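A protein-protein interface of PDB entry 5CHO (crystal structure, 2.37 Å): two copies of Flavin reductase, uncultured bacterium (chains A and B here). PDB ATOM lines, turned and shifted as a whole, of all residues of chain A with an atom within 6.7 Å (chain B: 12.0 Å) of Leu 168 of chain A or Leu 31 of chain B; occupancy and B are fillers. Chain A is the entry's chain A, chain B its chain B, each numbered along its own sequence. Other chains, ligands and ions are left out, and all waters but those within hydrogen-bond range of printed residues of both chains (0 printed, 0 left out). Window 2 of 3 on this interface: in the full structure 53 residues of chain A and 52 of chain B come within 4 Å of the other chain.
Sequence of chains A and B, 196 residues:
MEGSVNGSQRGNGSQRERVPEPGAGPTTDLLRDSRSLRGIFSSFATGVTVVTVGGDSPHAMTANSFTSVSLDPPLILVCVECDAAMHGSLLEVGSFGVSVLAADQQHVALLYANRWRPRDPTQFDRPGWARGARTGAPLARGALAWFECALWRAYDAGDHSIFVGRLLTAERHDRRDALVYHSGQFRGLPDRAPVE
No position is printed for both chains.
The backbone NH of Leu 167 of chain A is in hydrogen-bond range of the backbone carbonyl oxygen of Pro 74 of chain A, 2.9 Å away. The backbone NH (N) of Leu 168 of chain A lies within hydrogen-bond range of the backbone carbonyl oxygen (O) of Glu 148 of chain A (2.8 Å).
Of the 16 printed residues of chain A, 7 touch a printed residue of chain B. Along chain A the printed residues that touch a printed residue of chain B span positions 71 to 171. Hydrophobic or aromatic side chains of chain B that line the printed part of chain A: Leu 31, Leu 37, Ile 40 and Phe 41.
Among the printed residues, merely in contact across the chains: Leu 168 of chain A with Leu 31 of chain B, Ala 170 of chain A with Ile 40 of chain B, Leu 71 of chain A with Leu 37 of chain B, Phe 147 of chain A with Ile 40 of chain B, Glu 171 of chain A with Ile 40 of chain B, Ala 170 of chain A with Leu 31 of chain B, Leu 167 of chain A with Leu 37 of chain B, Phe 147 of chain A with Phe 41 of chain B, Leu 167 of chain A with Phe 41 of chain B, Leu 71 of chain A with Ser 34 of chain B, Pro 74 of chain A with Leu 37 of chain B and Leu 71 of chain A with Phe 41 of chain B.
The backbone NH (N) of Leu 71 of chain A sits at hydrogen-bond distance from the side-chain carboxylate (OD2) of Asp 159 of chain B, 2.9 Å away.
Printed residues of chain B within 4 Å of Leu 168 of chain A: Leu 31. Leu 31 of chain B touches just these residues of chain A: Leu 168 and Ala 170. Of chain B, only Leu 37 (3.9 Å) comes within 4 Å of Pro 74 of chain A. No residue of chain B comes within 4 Å of Arg 134 of chain A. No residue of chain B comes within 4 Å of Thr 135 of chain A. No residue of chain B comes within 4 Å of Glu 148 of chain A. No residue of chain B comes within 4 Å of Cys 149 of chain A. No residue of chain B comes within 4 Å of Arg 166 of chain A. Leu 167 of chain A touches two residues of chain B. No residue of chain B comes within 4 Å of Thr 169 of chain A. Of chain B, only Leu 31 and Ile 40 come within 4 Å of Ala 170 of chain A. Of the printed residues of chain B, Leu 71 of chain A touches Ser 34 (3.9 Å), Leu 37 (3.7 Å), Phe 41 (3.98 Å) and Asp 159 (2.9 Å). Of the printed residues of chain B, Phe 147 of chain A touches Ile 40 and Phe 41. Of the printed residues of chain A, Phe 41 of chain B touches Leu 71, Phe 147 and Leu 167. Arg 35 of chain B touches none of the printed residues of chain A. The nearest residue of chain A that does not touch Leu 31 of chain B is Thr 169 of chain A (4.1 Å). The nearest printed residue of chain A that does not touch Phe 41 of chain B is Pro 74 of chain A (5.7 Å).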
ATOM      1  N   LEU A  71      37.596  16.032  28.506  1.00  0.00           N
ATOM      2  CA  LEU A  71      37.042  15.712  29.816  1.00  0.00           C
ATOM      3  C   LEU A  71      37.010  16.925  30.716  1.00  0.00           C
ATOM      4  O   LEU A  71      36.109  17.071  31.538  1.00  0.00           O
ATOM      5  CB  LEU A  71      37.859  14.614  30.495  1.00  0.00           C
ATOM      6  CG  LEU A  71      37.629  13.199  29.973  1.00  0.00           C
ATOM      7  CD1 LEU A  71      38.656  12.210  30.530  1.00  0.00           C
ATOM      8  CD2 LEU A  71      36.211  12.787  30.318  1.00  0.00           C
ATOM      9  N   PRO A  74      34.265  19.154  29.929  1.00  0.00           N
ATOM     10  CA  PRO A  74      33.570  18.069  29.230  1.00  0.00           C
ATOM     11  C   PRO A  74      32.991  18.530  27.889  1.00  0.00           C
ATOM     12  O   PRO A  74      32.010  19.276  27.869  1.00  0.00           O
ATOM     13  CB  PRO A  74      32.461  17.681  30.209  1.00  0.00           C
ATOM     14  CG  PRO A  74      32.177  18.932  30.953  1.00  0.00           C
ATOM     15  CD  PRO A  74      33.488  19.656  31.074  1.00  0.00           C
ATOM     16  N   SER A  95      21.715  25.146  21.898  1.00  0.00           N
ATOM     17  CA  SER A  95      21.889  23.935  22.700  1.00  0.00           C
ATOM     18  C   SER A  95      21.256  22.746  21.990  1.00  0.00           C
ATOM     19  O   SER A  95      20.424  22.920  21.100  1.00  0.00           O
ATOM     20  CB  SER A  95      21.280  24.105  24.096  1.00  0.00           C
ATOM     21  OG  SER A  95      19.871  24.230  24.026  1.00  0.00           O
ATOM     22  N   PHE A  96      21.649  21.537  22.377  1.00  0.00           N
ATOM     23  CA  PHE A  96      21.154  20.351  21.696  1.00  0.00           C
ATOM     24  C   PHE A  96      21.301  19.073  22.510  1.00  0.00           C
ATOM     25  O   PHE A  96      22.042  19.018  23.493  1.00  0.00           O
ATOM     26  CB  PHE A  96      21.867  20.187  20.349  1.00  0.00           C
ATOM     27  CG  PHE A  96      23.354  20.022  20.457  1.00  0.00           C
ATOM     28  CD1 PHE A  96      23.926  18.755  20.470  1.00  0.00           C
ATOM     29  CD2 PHE A  96      24.186  21.132  20.513  1.00  0.00           C
ATOM     30  CE1 PHE A  96      25.302  18.600  20.551  1.00  0.00           C
ATOM     31  CE2 PHE A  96      25.557  20.984  20.594  1.00  0.00           C
ATOM     32  CZ  PHE A  96      26.117  19.717  20.614  1.00  0.00           C
ATOM     33  N   ARG A 134      17.523  20.226  30.990  1.00  0.00           N
ATOM     34  CA  ARG A 134      18.286  21.466  30.879  1.00  0.00           C
ATOM     35  C   ARG A 134      18.066  22.225  29.576  1.00  0.00           C
ATOM     36  O   ARG A 134      18.136  23.454  29.556  1.00  0.00           O
ATOM     37  CB  ARG A 134      19.779  21.174  31.028  1.00  0.00           C
ATOM     38  CG  ARG A 134      20.180  20.665  32.396  1.00  0.00           C
ATOM     39  CD  ARG A 134      20.001  21.755  33.445  1.00  0.00           C
ATOM     40  NE  ARG A 134      20.855  22.910  33.177  1.00  0.00           N
ATOM     41  CZ  ARG A 134      22.144  22.979  33.494  1.00  0.00           C
ATOM     42  NH1 ARG A 134      22.742  21.957  34.097  1.00  0.00           N
ATOM     43  NH2 ARG A 134      22.842  24.072  33.207  1.00  0.00           N
ATOM     44  N   THR A 135      17.790  21.499  28.498  1.00  0.00           N
ATOM     45  CA  THR A 135      17.729  22.095  27.166  1.00  0.00           C
ATOM     46  C   THR A 135      16.360  21.930  26.522  1.00  0.00           C
ATOM     47  O   THR A 135      16.050  22.602  25.541  1.00  0.00           O
ATOM     48  CB  THR A 135      18.785  21.468  26.242  1.00  0.00           C
ATOM     49  OG1 THR A 135      18.495  20.077  26.061  1.00  0.00           O
ATOM     50  CG2 THR A 135      20.174  21.626  26.844  1.00  0.00           C
ATOM     51  N   PHE A 147      22.911  12.736  26.163  1.00  0.00           N
ATOM     52  CA  PHE A 147      23.720  13.917  26.447  1.00  0.00           C
ATOM     53  C   PHE A 147      22.901  15.169  26.173  1.00  0.00           C
ATOM     54  O   PHE A 147      22.120  15.203  25.223  1.00  0.00           O
ATOM     55  CB  PHE A 147      24.993  13.980  25.594  1.00  0.00           C
ATOM     56  CG  PHE A 147      25.887  12.779  25.712  1.00  0.00           C
ATOM     57  CD1 PHE A 147      26.922  12.744  26.639  1.00  0.00           C
ATOM     58  CD2 PHE A 147      25.695  11.682  24.886  1.00  0.00           C
ATOM     59  CE1 PHE A 147      27.746  11.634  26.737  1.00  0.00           C
ATOM     60  CE2 PHE A 147      26.517  10.577  24.975  1.00  0.00           C
ATOM     61  CZ  PHE A 147      27.542  10.551  25.905  1.00  0.00           C
ATOM     62  N   GLU A 148      23.076  16.191  27.005  1.00  0.00           N
ATOM     63  CA  GLU A 148      22.625  17.539  26.669  1.00  0.00           C
ATOM     64  C   GLU A 148      23.843  18.436  26.588  1.00  0.00           C
ATOM     65  O   GLU A 148      24.759  18.326  27.404  1.00  0.00           O
ATOM     66  CB  GLU A 148      21.633  18.096  27.692  1.00  0.00           C
ATOM     67  CG  GLU A 148      20.324  17.341  27.788  1.00  0.00           C
ATOM     68  CD  GLU A 148      19.372  17.984  28.777  1.00  0.00           C
ATOM     69  OE1 GLU A 148      18.594  18.869  28.363  1.00  0.00           O
ATOM     70  OE2 GLU A 148      19.408  17.616  29.970  1.00  0.00           O
ATOM     71  N   CYS A 149      23.844  19.329  25.606  1.00  0.00           N
ATOM     72  CA  CYS A 149      25.011  20.148  25.333  1.00  0.00           C
ATOM     73  C   CYS A 149      24.639  21.589  25.048  1.00  0.00           C
ATOM     74  O   CYS A 149      23.563  21.873  24.524  1.00  0.00           O
ATOM     75  CB  CYS A 149      25.778  19.582  24.137  1.00  0.00           C
ATOM     76  SG  CYS A 149      26.100  17.805  24.218  1.00  0.00           S
ATOM     77  N   ALA A 150      25.543  22.491  25.407  1.00  0.00           N
ATOM     78  CA  ALA A 150      25.464  23.878  24.987  1.00  0.00           C
ATOM     79  C   ALA A 150      26.508  24.100  23.912  1.00  0.00           C
ATOM     80  O   ALA A 150      27.640  23.638  24.046  1.00  0.00           O
ATOM     81  CB  ALA A 150      25.689  24.806  26.151  1.00  0.00           C
ATOM     82  N   ARG A 166      29.632  21.786  24.947  1.00  0.00           N
ATOM     83  CA  ARG A 166      30.005  21.536  26.330  1.00  0.00           C
ATOM     84  C   ARG A 166      28.839  20.849  27.025  1.00  0.00           C
ATOM     85  O   ARG A 166      27.704  21.318  26.961  1.00  0.00           O
ATOM     86  CB  ARG A 166      30.386  22.820  27.071  1.00  0.00           C
ATOM     87  CG  ARG A 166      30.820  22.514  28.496  1.00  0.00           C
ATOM     88  CD  ARG A 166      31.177  23.720  29.339  1.00  0.00           C
ATOM     89  NE  ARG A 166      31.634  23.251  30.644  1.00  0.00           N
ATOM     90  CZ  ARG A 166      32.341  23.962  31.517  1.00  0.00           C
ATOM     91  NH1 ARG A 166      32.703  25.210  31.246  1.00  0.00           N
ATOM     92  NH2 ARG A 166      32.692  23.410  32.671  1.00  0.00           N
ATOM     93  N   LEU A 167      29.125  19.729  27.678  1.00  0.00           N
ATOM     94  CA  LEU A 167      28.085  18.924  28.299  1.00  0.00           C
ATOM     95  C   LEU A 167      27.437  19.650  29.473  1.00  0.00           C
ATOM     96  O   LEU A 167      28.130  20.234  30.306  1.00  0.00           O
ATOM     97  CB  LEU A 167      28.668  17.582  28.761  1.00  0.00           C
ATOM     98  CG  LEU A 167      29.197  16.686  27.632  1.00  0.00           C
ATOM     99  CD1 LEU A 167      29.703  15.344  28.144  1.00  0.00           C
ATOM    100  CD2 LEU A 167      28.130  16.484  26.576  1.00  0.00           C
ATOM    101  N   LEU A 168      26.107  19.603  29.530  1.00  0.00           N
ATOM    102  CA  LEU A 168      25.358  20.100  30.681  1.00  0.00           C
ATOM    103  C   LEU A 168      24.891  18.903  31.482  1.00  0.00           C
ATOM    104  O   LEU A 168      24.828  18.951  32.710  1.00  0.00           O
ATOM    105  CB  LEU A 168      24.162  20.951  30.256  1.00  0.00           C
ATOM    106  CG  LEU A 168      24.362  21.928  29.102  1.00  0.00           C
ATOM    107  CD1 LEU A 168      23.020  22.574  28.757  1.00  0.00           C
ATOM    108  CD2 LEU A 168      25.399  22.962  29.476  1.00  0.00           C
ATOM    109  N   THR A 169      24.564  17.831  30.770  1.00  0.00           N
ATOM    110  CA  THR A 169      24.219  16.566  31.395  1.00  0.00           C
ATOM    111  C   THR A 169      24.695  15.410  30.538  1.00  0.00           C
ATOM    112  O   THR A 169      24.913  15.546  29.334  1.00  0.00           O
ATOM    113  CB  THR A 169      22.699  16.399  31.616  1.00  0.00           C
ATOM    114  OG1 THR A 169      22.020  16.406  30.355  1.00  0.00           O
ATOM    115  CG2 THR A 169      22.148  17.506  32.500  1.00  0.00           C
ATOM    116  N   ALA A 170      24.845  14.267  31.185  1.00  0.00           N
ATOM    117  CA  ALA A 170      25.237  13.043  30.519  1.00  0.00           C
ATOM    118  C   ALA A 170      24.774  11.909  31.408  1.00  0.00           C
ATOM    119  O   ALA A 170      24.827  12.008  32.634  1.00  0.00           O
ATOM    120  CB  ALA A 170      26.735  12.993  30.284  1.00  0.00           C
ATOM    121  N   GLU A 171      24.327  10.830  30.784  1.00  0.00           N
ATOM    122  CA  GLU A 171      23.686   9.752  31.511  1.00  0.00           C
ATOM    123  C   GLU A 171      23.742   8.489  30.685  1.00  0.00           C
ATOM    124  O   GLU A 171      23.383   8.492  29.508  1.00  0.00           O
ATOM    125  CB  GLU A 171      22.231  10.102  31.823  1.00  0.00           C
ATOM    126  CG  GLU A 171      21.501   9.052  32.643  1.00  0.00           C
ATOM    127  CD  GLU A 171      20.035   9.387  32.832  1.00  0.00           C
ATOM    128  OE1 GLU A 171      19.607  10.471  32.381  1.00  0.00           O
ATOM    129  OE2 GLU A 171      19.308   8.566  33.427  1.00  0.00           O
ATOM    130  N   LEU B  31      29.715  14.531  36.288  1.00  0.00           N
ATOM    131  CA  LEU B  31      30.296  15.146  35.103  1.00  0.00           C
ATOM    132  C   LEU B  31      31.753  15.551  35.298  1.00  0.00           C
ATOM    133  O   LEU B  31      32.494  15.707  34.327  1.00  0.00           O
ATOM    134  CB  LEU B  31      29.470  16.370  34.707  1.00  0.00           C
ATOM    135  CG  LEU B  31      28.059  16.120  34.175  1.00  0.00           C
ATOM    136  CD1 LEU B  31      27.365  17.437  33.880  1.00  0.00           C
ATOM    137  CD2 LEU B  31      28.110  15.257  32.923  1.00  0.00           C
ATOM    138  N   ARG B  32      32.160  15.732  36.549  1.00  0.00           N
ATOM    139  CA  ARG B  32      33.542  16.078  36.862  1.00  0.00           C
ATOM    140  C   ARG B  32      34.382  14.809  36.990  1.00  0.00           C
ATOM    141  O   ARG B  32      35.613  14.863  37.000  1.00  0.00           O
ATOM    142  CB  ARG B  32      33.622  16.900  38.147  1.00  0.00           C
ATOM    143  N   ASP B  33      33.704  13.667  37.069  1.00  0.00           N
ATOM    144  CA  ASP B  33      34.373  12.393  37.293  1.00  0.00           C
ATOM    145  C   ASP B  33      34.763  11.759  35.963  1.00  0.00           C
ATOM    146  O   ASP B  33      33.915  11.494  35.111  1.00  0.00           O
ATOM    147  CB  ASP B  33      33.465  11.454  38.092  1.00  0.00           C
ATOM    148  CG  ASP B  33      34.123  10.120  38.392  1.00  0.00           C
ATOM    149  OD1 ASP B  33      35.369  10.039  38.334  1.00  0.00           O
ATOM    150  OD2 ASP B  33      33.393   9.151  38.691  1.00  0.00           O
ATOM    151  N   SER B  34      36.059  11.516  35.807  1.00  0.00           N
ATOM    152  CA  SER B  34      36.614  10.996  34.565  1.00  0.00           C
ATOM    153  C   SER B  34      36.208   9.549  34.304  1.00  0.00           C
ATOM    154  O   SER B  34      35.881   9.184  33.173  1.00  0.00           O
ATOM    155  CB  SER B  34      38.139  11.103  34.587  1.00  0.00           C
ATOM    156  OG  SER B  34      38.562  12.439  34.383  1.00  0.00           O
ATOM    157  N   ARG B  35      36.226   8.726  35.347  1.00  0.00           N
ATOM    158  CA  ARG B  35      35.946   7.304  35.186  1.00  0.00           C
ATOM    159  C   ARG B  35      34.488   7.124  34.777  1.00  0.00           C
ATOM    160  O   ARG B  35      34.163   6.277  33.942  1.00  0.00           O
ATOM    161  CB  ARG B  35      36.243   6.545  36.482  1.00  0.00           C
ATOM    162  N   SER B  36      33.616   7.938  35.363  1.00  0.00           N
ATOM    163  CA  SER B  36      32.187   7.875  35.074  1.00  0.00           C
ATOM    164  C   SER B  36      31.866   8.375  33.665  1.00  0.00           C
ATOM    165  O   SER B  36      31.193   7.698  32.889  1.00  0.00           O
ATOM    166  CB  SER B  36      31.403   8.694  36.099  1.00  0.00           C
ATOM    167  OG  SER B  36      30.047   8.819  35.707  1.00  0.00           O
ATOM    168  N   LEU B  37      32.371   9.562  33.341  1.00  0.00           N
ATOM    169  CA  LEU B  37      32.098  10.199  32.055  1.00  0.00           C
ATOM    170  C   LEU B  37      32.707   9.396  30.915  1.00  0.00           C
ATOM    171  O   LEU B  37      32.108   9.283  29.845  1.00  0.00           O
ATOM    172  CB  LEU B  37      32.634  11.633  32.046  1.00  0.00           C
ATOM    173  CG  LEU B  37      32.318  12.558  30.864  1.00  0.00           C
ATOM    174  CD1 LEU B  37      30.834  12.620  30.508  1.00  0.00           C
ATOM    175  CD2 LEU B  37      32.840  13.949  31.198  1.00  0.00           C
ATOM    176  N   ARG B  38      33.902   8.858  31.143  1.00  0.00           N
ATOM    177  CA  ARG B  38      34.545   7.990  30.164  1.00  0.00           C
ATOM    178  C   ARG B  38      33.648   6.783  29.915  1.00  0.00           C
ATOM    179  O   ARG B  38      33.583   6.266  28.802  1.00  0.00           O
ATOM    180  CB  ARG B  38      35.927   7.539  30.647  1.00  0.00           C
ATOM    181  N   GLY B  39      32.957   6.349  30.965  1.00  0.00           N
ATOM    182  CA  GLY B  39      32.020   5.242  30.873  1.00  0.00           C
ATOM    183  C   GLY B  39      30.810   5.538  30.002  1.00  0.00           C
ATOM    184  O   GLY B  39      30.361   4.681  29.242  1.00  0.00           O
ATOM    185  N   ILE B  40      30.273   6.749  30.110  1.00  0.00           N
ATOM    186  CA  ILE B  40      29.120   7.129  29.301  1.00  0.00           C
ATOM    187  C   ILE B  40      29.560   7.247  27.842  1.00  0.00           C
ATOM    188  O   ILE B  40      28.905   6.716  26.944  1.00  0.00           O
ATOM    189  CB  ILE B  40      28.474   8.459  29.754  1.00  0.00           C
ATOM    190  CG1 ILE B  40      28.321   8.499  31.280  1.00  0.00           C
ATOM    191  CG2 ILE B  40      27.122   8.645  29.051  1.00  0.00           C
ATOM    192  CD1 ILE B  40      27.737   9.794  31.820  1.00  0.00           C
ATOM    193  N   PHE B  41      30.661   7.963  27.618  1.00  0.00           N
ATOM    194  CA  PHE B  41      31.287   8.032  26.301  1.00  0.00           C
ATOM    195  C   PHE B  41      31.475   6.669  25.650  1.00  0.00           C
ATOM    196  O   PHE B  41      31.357   6.549  24.433  1.00  0.00           O
ATOM    197  CB  PHE B  41      32.663   8.703  26.387  1.00  0.00           C
ATOM    198  CG  PHE B  41      32.630  10.197  26.594  1.00  0.00           C
ATOM    199  CD1 PHE B  41      31.488  10.950  26.358  1.00  0.00           C
ATOM    200  CD2 PHE B  41      33.774  10.848  27.022  1.00  0.00           C
ATOM    201  CE1 PHE B  41      31.498  12.322  26.548  1.00  0.00           C
ATOM    202  CE2 PHE B  41      33.788  12.214  27.215  1.00  0.00           C
ATOM    203  CZ  PHE B  41      32.651  12.952  26.980  1.00  0.00           C
ATOM    204  N   ASP B 159      40.938  19.961  26.736  1.00  0.00           N
ATOM    205  CA  ASP B 159      42.193  19.257  26.991  1.00  0.00           C
ATOM    206  C   ASP B 159      42.700  18.468  25.775  1.00  0.00           C
ATOM    207  O   ASP B 159      43.732  17.797  25.856  1.00  0.00           O
ATOM    208  CB  ASP B 159      42.033  18.327  28.202  1.00  0.00           C
ATOM    209  CG  ASP B 159      40.918  17.311  28.028  1.00  0.00           C
ATOM    210  OD1 ASP B 159      40.643  16.896  26.883  1.00  0.00           O
ATOM    211  OD2 ASP B 159      40.303  16.926  29.044  1.00  0.00           O
